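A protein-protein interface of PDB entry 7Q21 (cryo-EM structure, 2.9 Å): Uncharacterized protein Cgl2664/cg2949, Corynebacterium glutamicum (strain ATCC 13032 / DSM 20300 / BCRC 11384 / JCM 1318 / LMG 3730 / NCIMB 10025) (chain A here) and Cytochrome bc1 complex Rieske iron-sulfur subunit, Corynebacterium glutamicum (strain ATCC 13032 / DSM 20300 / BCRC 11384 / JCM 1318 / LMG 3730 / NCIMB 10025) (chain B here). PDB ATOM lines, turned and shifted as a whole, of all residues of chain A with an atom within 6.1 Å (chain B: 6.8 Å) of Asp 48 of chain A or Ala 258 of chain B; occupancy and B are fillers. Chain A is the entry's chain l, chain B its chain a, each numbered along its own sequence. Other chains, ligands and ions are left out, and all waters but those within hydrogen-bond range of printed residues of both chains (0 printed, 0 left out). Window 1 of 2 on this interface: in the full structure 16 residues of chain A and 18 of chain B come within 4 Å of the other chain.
Of the printed residues of chain B, Val 47 of chain A touches Arg 305. Asp 63 of chain A touches none of the printed residues of chain B. Printed residues of chain B within 4 Å of Thr 169 of chain A: Arg 303, Thr 306 and Asp 325. Printed residues of chain B within 4 Å of Ser 171 of chain A: Arg 303 (3.9 Å). Of the printed residues of chain A, Ala 258 of chain B touches Asp 48. Printed residues of chain A within 4 Å of Arg 305 of chain B: Ala 46 and Val 47. Tyr 343 of chain B touches none of the printed residues of chain A. The nearest residue of chain B that does not touch Asp 48 of chain A is Ala 257 of chain B (4.04 Å). The nearest residue of chain A that does not touch Ala 258 of chain B is Val 47 of chain A (4.2 Å).
Among the printed residues, pairs that only touch across the chains: Ala 46 of chain A with Arg 305 of chain B (3.9 Å), Val 47 of chain A with Arg 305 of chain B (3.9 Å), Thr 169 of chain A with Thr 306 of chain B (3.5 Å), Thr 169 of chain A with Asp 325 of chain B (3.8 Å) and Ser 171 of chain A with Arg 303 of chain B (3.9 Å).
Of the 13 printed residues of chain A, 5 touch a printed residue of chain B. Printed residues of chain A that touch a printed residue of chain B: Ala 46, Val 47, Asp 48, Thr 169 and Ser 171. Printed residues of chain B that touch a printed residue of chain A: Ala 258, Arg 303, Arg 305, Thr 306 and Asp 325. Along chain B the printed residues that touch a printed residue of chain A span positions 258 to 325.
N of Leu 304 of chain B lies within hydrogen-bond range of O of Asp 325 of chain B (3.1 Å). The guanidinium group (NH2) of Arg 303 of chain B is in hydrogen-bond range of the backbone carbonyl oxygen (O) of Leu 256 of chain B (2.7 Å). N of Ala 259 of chain B is in hydrogen-bond range of O of Arg 303 of chain B (2.7 Å). N of Arg 303 of chain B lies within hydrogen-bond range of O of Ser 260 of chain B (3.0 Å). O of Asp 48 of chain A sits close to OD1 of Asp 63 of chain A (2.7 Å).
NH1 of Arg 303 of chain B lies within hydrogen-bond range of OG1 of Thr 169 of chain A (2.9 Å). The backbone NH (N) of Ala 258 of chain B is in hydrogen-bond range of the side-chain carboxylate (OD1) of Asp 48 of chain A (3.0 Å).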
ATOM      1  N   ALA A  46     -17.599  11.762  -5.589  1.00  0.00           N
ATOM      2  CA  ALA A  46     -17.046  11.350  -6.876  1.00  0.00           C
ATOM      3  C   ALA A  46     -16.004  10.246  -6.694  1.00  0.00           C
ATOM      4  O   ALA A  46     -14.926  10.290  -7.283  1.00  0.00           O
ATOM      5  CB  ALA A  46     -16.505  12.536  -7.646  1.00  0.00           C
ATOM      6  N   VAL A  47     -16.352   9.267  -5.853  1.00  0.00           N
ATOM      7  CA  VAL A  47     -15.552   8.073  -5.624  1.00  0.00           C
ATOM      8  C   VAL A  47     -16.464   6.859  -5.782  1.00  0.00           C
ATOM      9  O   VAL A  47     -17.643   7.005  -6.099  1.00  0.00           O
ATOM     10  CB  VAL A  47     -14.868   8.098  -4.242  1.00  0.00           C
ATOM     11  CG1 VAL A  47     -13.844   9.216  -4.125  1.00  0.00           C
ATOM     12  CG2 VAL A  47     -15.869   8.159  -3.098  1.00  0.00           C
ATOM     13  N   ASP A  48     -15.914   5.666  -5.531  1.00  0.00           N
ATOM     14  CA  ASP A  48     -16.686   4.435  -5.604  1.00  0.00           C
ATOM     15  C   ASP A  48     -17.242   4.115  -4.220  1.00  0.00           C
ATOM     16  O   ASP A  48     -16.492   3.983  -3.256  1.00  0.00           O
ATOM     17  CB  ASP A  48     -15.867   3.269  -6.168  1.00  0.00           C
ATOM     18  CG  ASP A  48     -15.228   3.523  -7.527  1.00  0.00           C
ATOM     19  OD1 ASP A  48     -15.854   4.208  -8.366  1.00  0.00           O
ATOM     20  OD2 ASP A  48     -14.101   3.022  -7.741  1.00  0.00           O
ATOM     21  N   GLY A  49     -18.571   3.994  -4.145  1.00  0.00           N
ATOM     22  CA  GLY A  49     -19.232   3.572  -2.922  1.00  0.00           C
ATOM     23  C   GLY A  49     -19.781   4.745  -2.121  1.00  0.00           C
ATOM     24  O   GLY A  49     -19.106   5.759  -1.954  1.00  0.00           O
ATOM     25  N   ASN A  50     -21.002   4.565  -1.613  1.00  0.00           N
ATOM     26  CA  ASN A  50     -21.808   5.631  -1.042  1.00  0.00           C
ATOM     27  C   ASN A  50     -21.543   5.736   0.456  1.00  0.00           C
ATOM     28  O   ASN A  50     -20.654   5.073   0.985  1.00  0.00           O
ATOM     29  CB  ASN A  50     -23.291   5.403  -1.347  1.00  0.00           C
ATOM     30  CG  ASN A  50     -23.747   3.995  -1.023  1.00  0.00           C
ATOM     31  OD1 ASN A  50     -22.931   3.110  -0.767  1.00  0.00           O
ATOM     32  ND2 ASN A  50     -25.051   3.779  -1.036  1.00  0.00           N
ATOM     33  N   ASP A  63     -17.311   6.152   1.949  1.00  0.00           N
ATOM     34  CA  ASP A  63     -16.594   5.461   0.886  1.00  0.00           C
ATOM     35  C   ASP A  63     -16.591   3.955   1.146  1.00  0.00           C
ATOM     36  O   ASP A  63     -15.562   3.357   1.467  1.00  0.00           O
ATOM     37  CB  ASP A  63     -15.232   6.111   0.627  1.00  0.00           C
ATOM     38  CG  ASP A  63     -14.342   5.332  -0.325  1.00  0.00           C
ATOM     39  OD1 ASP A  63     -14.806   5.005  -1.435  1.00  0.00           O
ATOM     40  OD2 ASP A  63     -13.201   5.041   0.064  1.00  0.00           O
ATOM     41  N   VAL A  64     -17.778   3.362   1.004  1.00  0.00           N
ATOM     42  CA  VAL A  64     -17.990   1.965   1.332  1.00  0.00           C
ATOM     43  C   VAL A  64     -18.171   1.175   0.043  1.00  0.00           C
ATOM     44  O   VAL A  64     -19.141   1.381  -0.683  1.00  0.00           O
ATOM     45  CB  VAL A  64     -19.184   1.767   2.283  1.00  0.00           C
ATOM     46  CG1 VAL A  64     -19.325   0.312   2.698  1.00  0.00           C
ATOM     47  CG2 VAL A  64     -19.094   2.671   3.503  1.00  0.00           C
ATOM     48  N   THR A  65     -17.223   0.269  -0.212  1.00  0.00           N
ATOM     49  CA  THR A  65     -17.357  -0.713  -1.276  1.00  0.00           C
ATOM     50  C   THR A  65     -16.909  -2.082  -0.780  1.00  0.00           C
ATOM     51  O   THR A  65     -16.355  -2.217   0.312  1.00  0.00           O
ATOM     52  CB  THR A  65     -16.557  -0.346  -2.536  1.00  0.00           C
ATOM     53  OG1 THR A  65     -15.170  -0.214  -2.218  1.00  0.00           O
ATOM     54  CG2 THR A  65     -17.066   0.889  -3.240  1.00  0.00           C
ATOM     55  N   HIS A  67     -14.270  -4.354  -2.088  1.00  0.00           N
ATOM     56  CA  HIS A  67     -13.127  -4.541  -2.965  1.00  0.00           C
ATOM     57  C   HIS A  67     -12.927  -6.025  -3.239  1.00  0.00           C
ATOM     58  O   HIS A  67     -13.026  -6.851  -2.332  1.00  0.00           O
ATOM     59  CB  HIS A  67     -11.855  -3.916  -2.386  1.00  0.00           C
ATOM     60  CG  HIS A  67     -11.801  -2.434  -2.519  1.00  0.00           C
ATOM     61  ND1 HIS A  67     -11.677  -1.795  -3.737  1.00  0.00           N
ATOM     62  CD2 HIS A  67     -11.840  -1.464  -1.584  1.00  0.00           C
ATOM     63  CE1 HIS A  67     -11.653  -0.491  -3.546  1.00  0.00           C
ATOM     64  NE2 HIS A  67     -11.749  -0.263  -2.231  1.00  0.00           N
ATOM     65  N   THR A 169     -21.369  -1.034  -3.861  1.00  0.00           N
ATOM     66  CA  THR A 169     -20.965  -1.620  -5.129  1.00  0.00           C
ATOM     67  C   THR A 169     -19.760  -2.535  -4.931  1.00  0.00           C
ATOM     68  O   THR A 169     -19.003  -2.383  -3.974  1.00  0.00           O
ATOM     69  CB  THR A 169     -20.693  -0.552  -6.197  1.00  0.00           C
ATOM     70  OG1 THR A 169     -20.546  -1.235  -7.441  1.00  0.00           O
ATOM     71  CG2 THR A 169     -19.439   0.255  -5.942  1.00  0.00           C
ATOM     72  N   SER A 171     -16.278  -3.493  -6.649  1.00  0.00           N
ATOM     73  CA  SER A 171     -15.330  -2.929  -7.594  1.00  0.00           C
ATOM     74  C   SER A 171     -13.917  -3.412  -7.288  1.00  0.00           C
ATOM     75  O   SER A 171     -13.621  -3.815  -6.164  1.00  0.00           O
ATOM     76  CB  SER A 171     -15.413  -1.421  -7.610  1.00  0.00           C
ATOM     77  OG  SER A 171     -15.419  -0.902  -6.289  1.00  0.00           O
ATOM     78  N   ALA A 172     -13.060  -3.358  -8.314  1.00  0.00           N
ATOM     79  CA  ALA A 172     -11.644  -3.656  -8.192  1.00  0.00           C
ATOM     80  C   ALA A 172     -10.928  -2.459  -7.568  1.00  0.00           C
ATOM     81  O   ALA A 172     -11.324  -1.319  -7.807  1.00  0.00           O
ATOM     82  CB  ALA A 172     -11.080  -3.992  -9.550  1.00  0.00           C
ATOM     83  N   VAL A 174      -8.112   0.533  -6.936  1.00  0.00           N
ATOM     84  CA  VAL A 174      -7.481   1.481  -7.843  1.00  0.00           C
ATOM     85  C   VAL A 174      -6.082   0.970  -8.184  1.00  0.00           C
ATOM     86  O   VAL A 174      -5.369   0.479  -7.311  1.00  0.00           O
ATOM     87  CB  VAL A 174      -7.456   2.901  -7.238  1.00  0.00           C
ATOM     88  CG1 VAL A 174      -6.736   3.906  -8.125  1.00  0.00           C
ATOM     89  CG2 VAL A 174      -8.854   3.403  -6.907  1.00  0.00           C
ATOM     90  N   LEU B 256     -14.461  -0.052 -15.455  1.00  0.00           N
ATOM     91  CA  LEU B 256     -15.132   1.235 -15.499  1.00  0.00           C
ATOM     92  C   LEU B 256     -15.467   1.673 -14.074  1.00  0.00           C
ATOM     93  O   LEU B 256     -16.107   0.933 -13.331  1.00  0.00           O
ATOM     94  CB  LEU B 256     -16.390   1.049 -16.353  1.00  0.00           C
ATOM     95  CG  LEU B 256     -17.060   2.317 -16.889  1.00  0.00           C
ATOM     96  CD1 LEU B 256     -16.152   3.048 -17.859  1.00  0.00           C
ATOM     97  CD2 LEU B 256     -18.373   1.985 -17.582  1.00  0.00           C
ATOM     98  N   ALA B 257     -14.999   2.872 -13.710  1.00  0.00           N
ATOM     99  CA  ALA B 257     -15.226   3.450 -12.394  1.00  0.00           C
ATOM    100  C   ALA B 257     -16.611   4.090 -12.336  1.00  0.00           C
ATOM    101  O   ALA B 257     -17.187   4.429 -13.368  1.00  0.00           O
ATOM    102  CB  ALA B 257     -14.138   4.447 -12.079  1.00  0.00           C
ATOM    103  N   ALA B 258     -17.136   4.253 -11.113  1.00  0.00           N
ATOM    104  CA  ALA B 258     -18.455   4.832 -10.915  1.00  0.00           C
ATOM    105  C   ALA B 258     -18.460   6.279 -11.404  1.00  0.00           C
ATOM    106  O   ALA B 258     -17.476   6.998 -11.230  1.00  0.00           O
ATOM    107  CB  ALA B 258     -18.858   4.728  -9.466  1.00  0.00           C
ATOM    108  N   ALA B 259     -19.587   6.676 -12.015  1.00  0.00           N
ATOM    109  CA  ALA B 259     -19.753   7.956 -12.693  1.00  0.00           C
ATOM    110  C   ALA B 259     -18.746   8.093 -13.837  1.00  0.00           C
ATOM    111  O   ALA B 259     -17.921   9.006 -13.850  1.00  0.00           O
ATOM    112  CB  ALA B 259     -19.703   9.106 -11.713  1.00  0.00           C
ATOM    113  N   SER B 260     -18.816   7.157 -14.792  1.00  0.00           N
ATOM    114  CA  SER B 260     -17.999   7.217 -15.992  1.00  0.00           C
ATOM    115  C   SER B 260     -18.809   6.771 -17.203  1.00  0.00           C
ATOM    116  O   SER B 260     -19.830   6.097 -17.071  1.00  0.00           O
ATOM    117  CB  SER B 260     -16.755   6.397 -15.855  1.00  0.00           C
ATOM    118  OG  SER B 260     -17.107   5.059 -15.633  1.00  0.00           O
ATOM    119  N   ARG B 303     -21.547   3.816 -16.168  1.00  0.00           N
ATOM    120  CA  ARG B 303     -21.609   3.274 -14.824  1.00  0.00           C
ATOM    121  C   ARG B 303     -21.996   4.400 -13.875  1.00  0.00           C
ATOM    122  O   ARG B 303     -21.255   5.370 -13.730  1.00  0.00           O
ATOM    123  CB  ARG B 303     -20.308   2.595 -14.394  1.00  0.00           C
ATOM    124  CG  ARG B 303     -20.422   1.931 -13.030  1.00  0.00           C
ATOM    125  CD  ARG B 303     -19.217   1.098 -12.682  1.00  0.00           C
ATOM    126  NE  ARG B 303     -19.394   0.406 -11.413  1.00  0.00           N
ATOM    127  CZ  ARG B 303     -18.466  -0.331 -10.804  1.00  0.00           C
ATOM    128  NH1 ARG B 303     -18.743  -0.918  -9.653  1.00  0.00           N
ATOM    129  NH2 ARG B 303     -17.267  -0.481 -11.340  1.00  0.00           N
ATOM    130  N   LEU B 304     -23.160   4.235 -13.241  1.00  0.00           N
ATOM    131  CA  LEU B 304     -23.682   5.207 -12.299  1.00  0.00           C
ATOM    132  C   LEU B 304     -23.060   4.981 -10.926  1.00  0.00           C
ATOM    133  O   LEU B 304     -22.673   3.863 -10.584  1.00  0.00           O
ATOM    134  CB  LEU B 304     -25.204   5.053 -12.208  1.00  0.00           C
ATOM    135  CG  LEU B 304     -26.032   5.539 -13.393  1.00  0.00           C
ATOM    136  CD1 LEU B 304     -27.505   5.474 -13.048  1.00  0.00           C
ATOM    137  CD2 LEU B 304     -25.653   6.953 -13.801  1.00  0.00           C
ATOM    138  N   ARG B 305     -23.003   6.054 -10.130  1.00  0.00           N
ATOM    139  CA  ARG B 305     -22.684   5.957  -8.715  1.00  0.00           C
ATOM    140  C   ARG B 305     -23.771   5.159  -7.999  1.00  0.00           C
ATOM    141  O   ARG B 305     -24.931   5.178  -8.399  1.00  0.00           O
ATOM    142  CB  ARG B 305     -22.533   7.357  -8.118  1.00  0.00           C
ATOM    143  CG  ARG B 305     -21.402   7.456  -7.110  1.00  0.00           C
ATOM    144  CD  ARG B 305     -21.179   8.883  -6.653  1.00  0.00           C
ATOM    145  NE  ARG B 305     -20.511   9.720  -7.641  1.00  0.00           N
ATOM    146  CZ  ARG B 305     -21.113  10.598  -8.437  1.00  0.00           C
ATOM    147  NH1 ARG B 305     -20.396  11.324  -9.278  1.00  0.00           N
ATOM    148  NH2 ARG B 305     -22.423  10.762  -8.388  1.00  0.00           N
ATOM    149  N   THR B 306     -23.371   4.451  -6.939  1.00  0.00           N
ATOM    150  CA  THR B 306     -24.242   3.533  -6.218  1.00  0.00           C
ATOM    151  C   THR B 306     -25.476   4.254  -5.678  1.00  0.00           C
ATOM    152  O   THR B 306     -26.554   3.673  -5.622  1.00  0.00           O
ATOM    153  CB  THR B 306     -23.515   2.883  -5.034  1.00  0.00           C
ATOM    154  OG1 THR B 306     -22.214   2.457  -5.442  1.00  0.00           O
ATOM    155  CG2 THR B 306     -24.279   1.723  -4.439  1.00  0.00           C
ATOM    156  N   ASP B 325     -24.849  -1.796 -12.100  1.00  0.00           N
ATOM    157  CA  ASP B 325     -24.826  -0.345 -12.071  1.00  0.00           C
ATOM    158  C   ASP B 325     -24.655   0.236 -13.473  1.00  0.00           C
ATOM    159  O   ASP B 325     -24.525   1.450 -13.629  1.00  0.00           O
ATOM    160  CB  ASP B 325     -23.714   0.149 -11.144  1.00  0.00           C
ATOM    161  CG  ASP B 325     -24.155   0.303  -9.698  1.00  0.00           C
ATOM    162  OD1 ASP B 325     -25.310  -0.044  -9.386  1.00  0.00           O
ATOM    163  OD2 ASP B 325     -23.346   0.814  -8.895  1.00  0.00           O
ATOM    164  N   TYR B 343     -21.782  13.681 -21.347  1.00  0.00           N
ATOM    165  CA  TYR B 343     -22.362  13.133 -20.133  1.00  0.00           C
ATOM    166  C   TYR B 343     -21.812  13.867 -18.914  1.00  0.00           C
ATOM    167  O   TYR B 343     -20.610  13.835 -18.651  1.00  0.00           O
ATOM    168  CB  TYR B 343     -22.109  11.626 -20.056  1.00  0.00           C
ATOM    169  CG  TYR B 343     -22.358  11.027 -18.695  1.00  0.00           C
ATOM    170  CD1 TYR B 343     -23.641  10.951 -18.171  1.00  0.00           C
ATOM    171  CD2 TYR B 343     -21.309  10.545 -17.930  1.00  0.00           C
ATOM    172  CE1 TYR B 343     -23.875  10.413 -16.914  1.00  0.00           C
ATOM    173  CE2 TYR B 343     -21.526   9.999 -16.675  1.00  0.00           C
ATOM    174  CZ  TYR B 343     -22.813   9.935 -16.165  1.00  0.00           C
ATOM    175  OH  TYR B 343     -23.021   9.395 -14.929  1.00  0.00           O
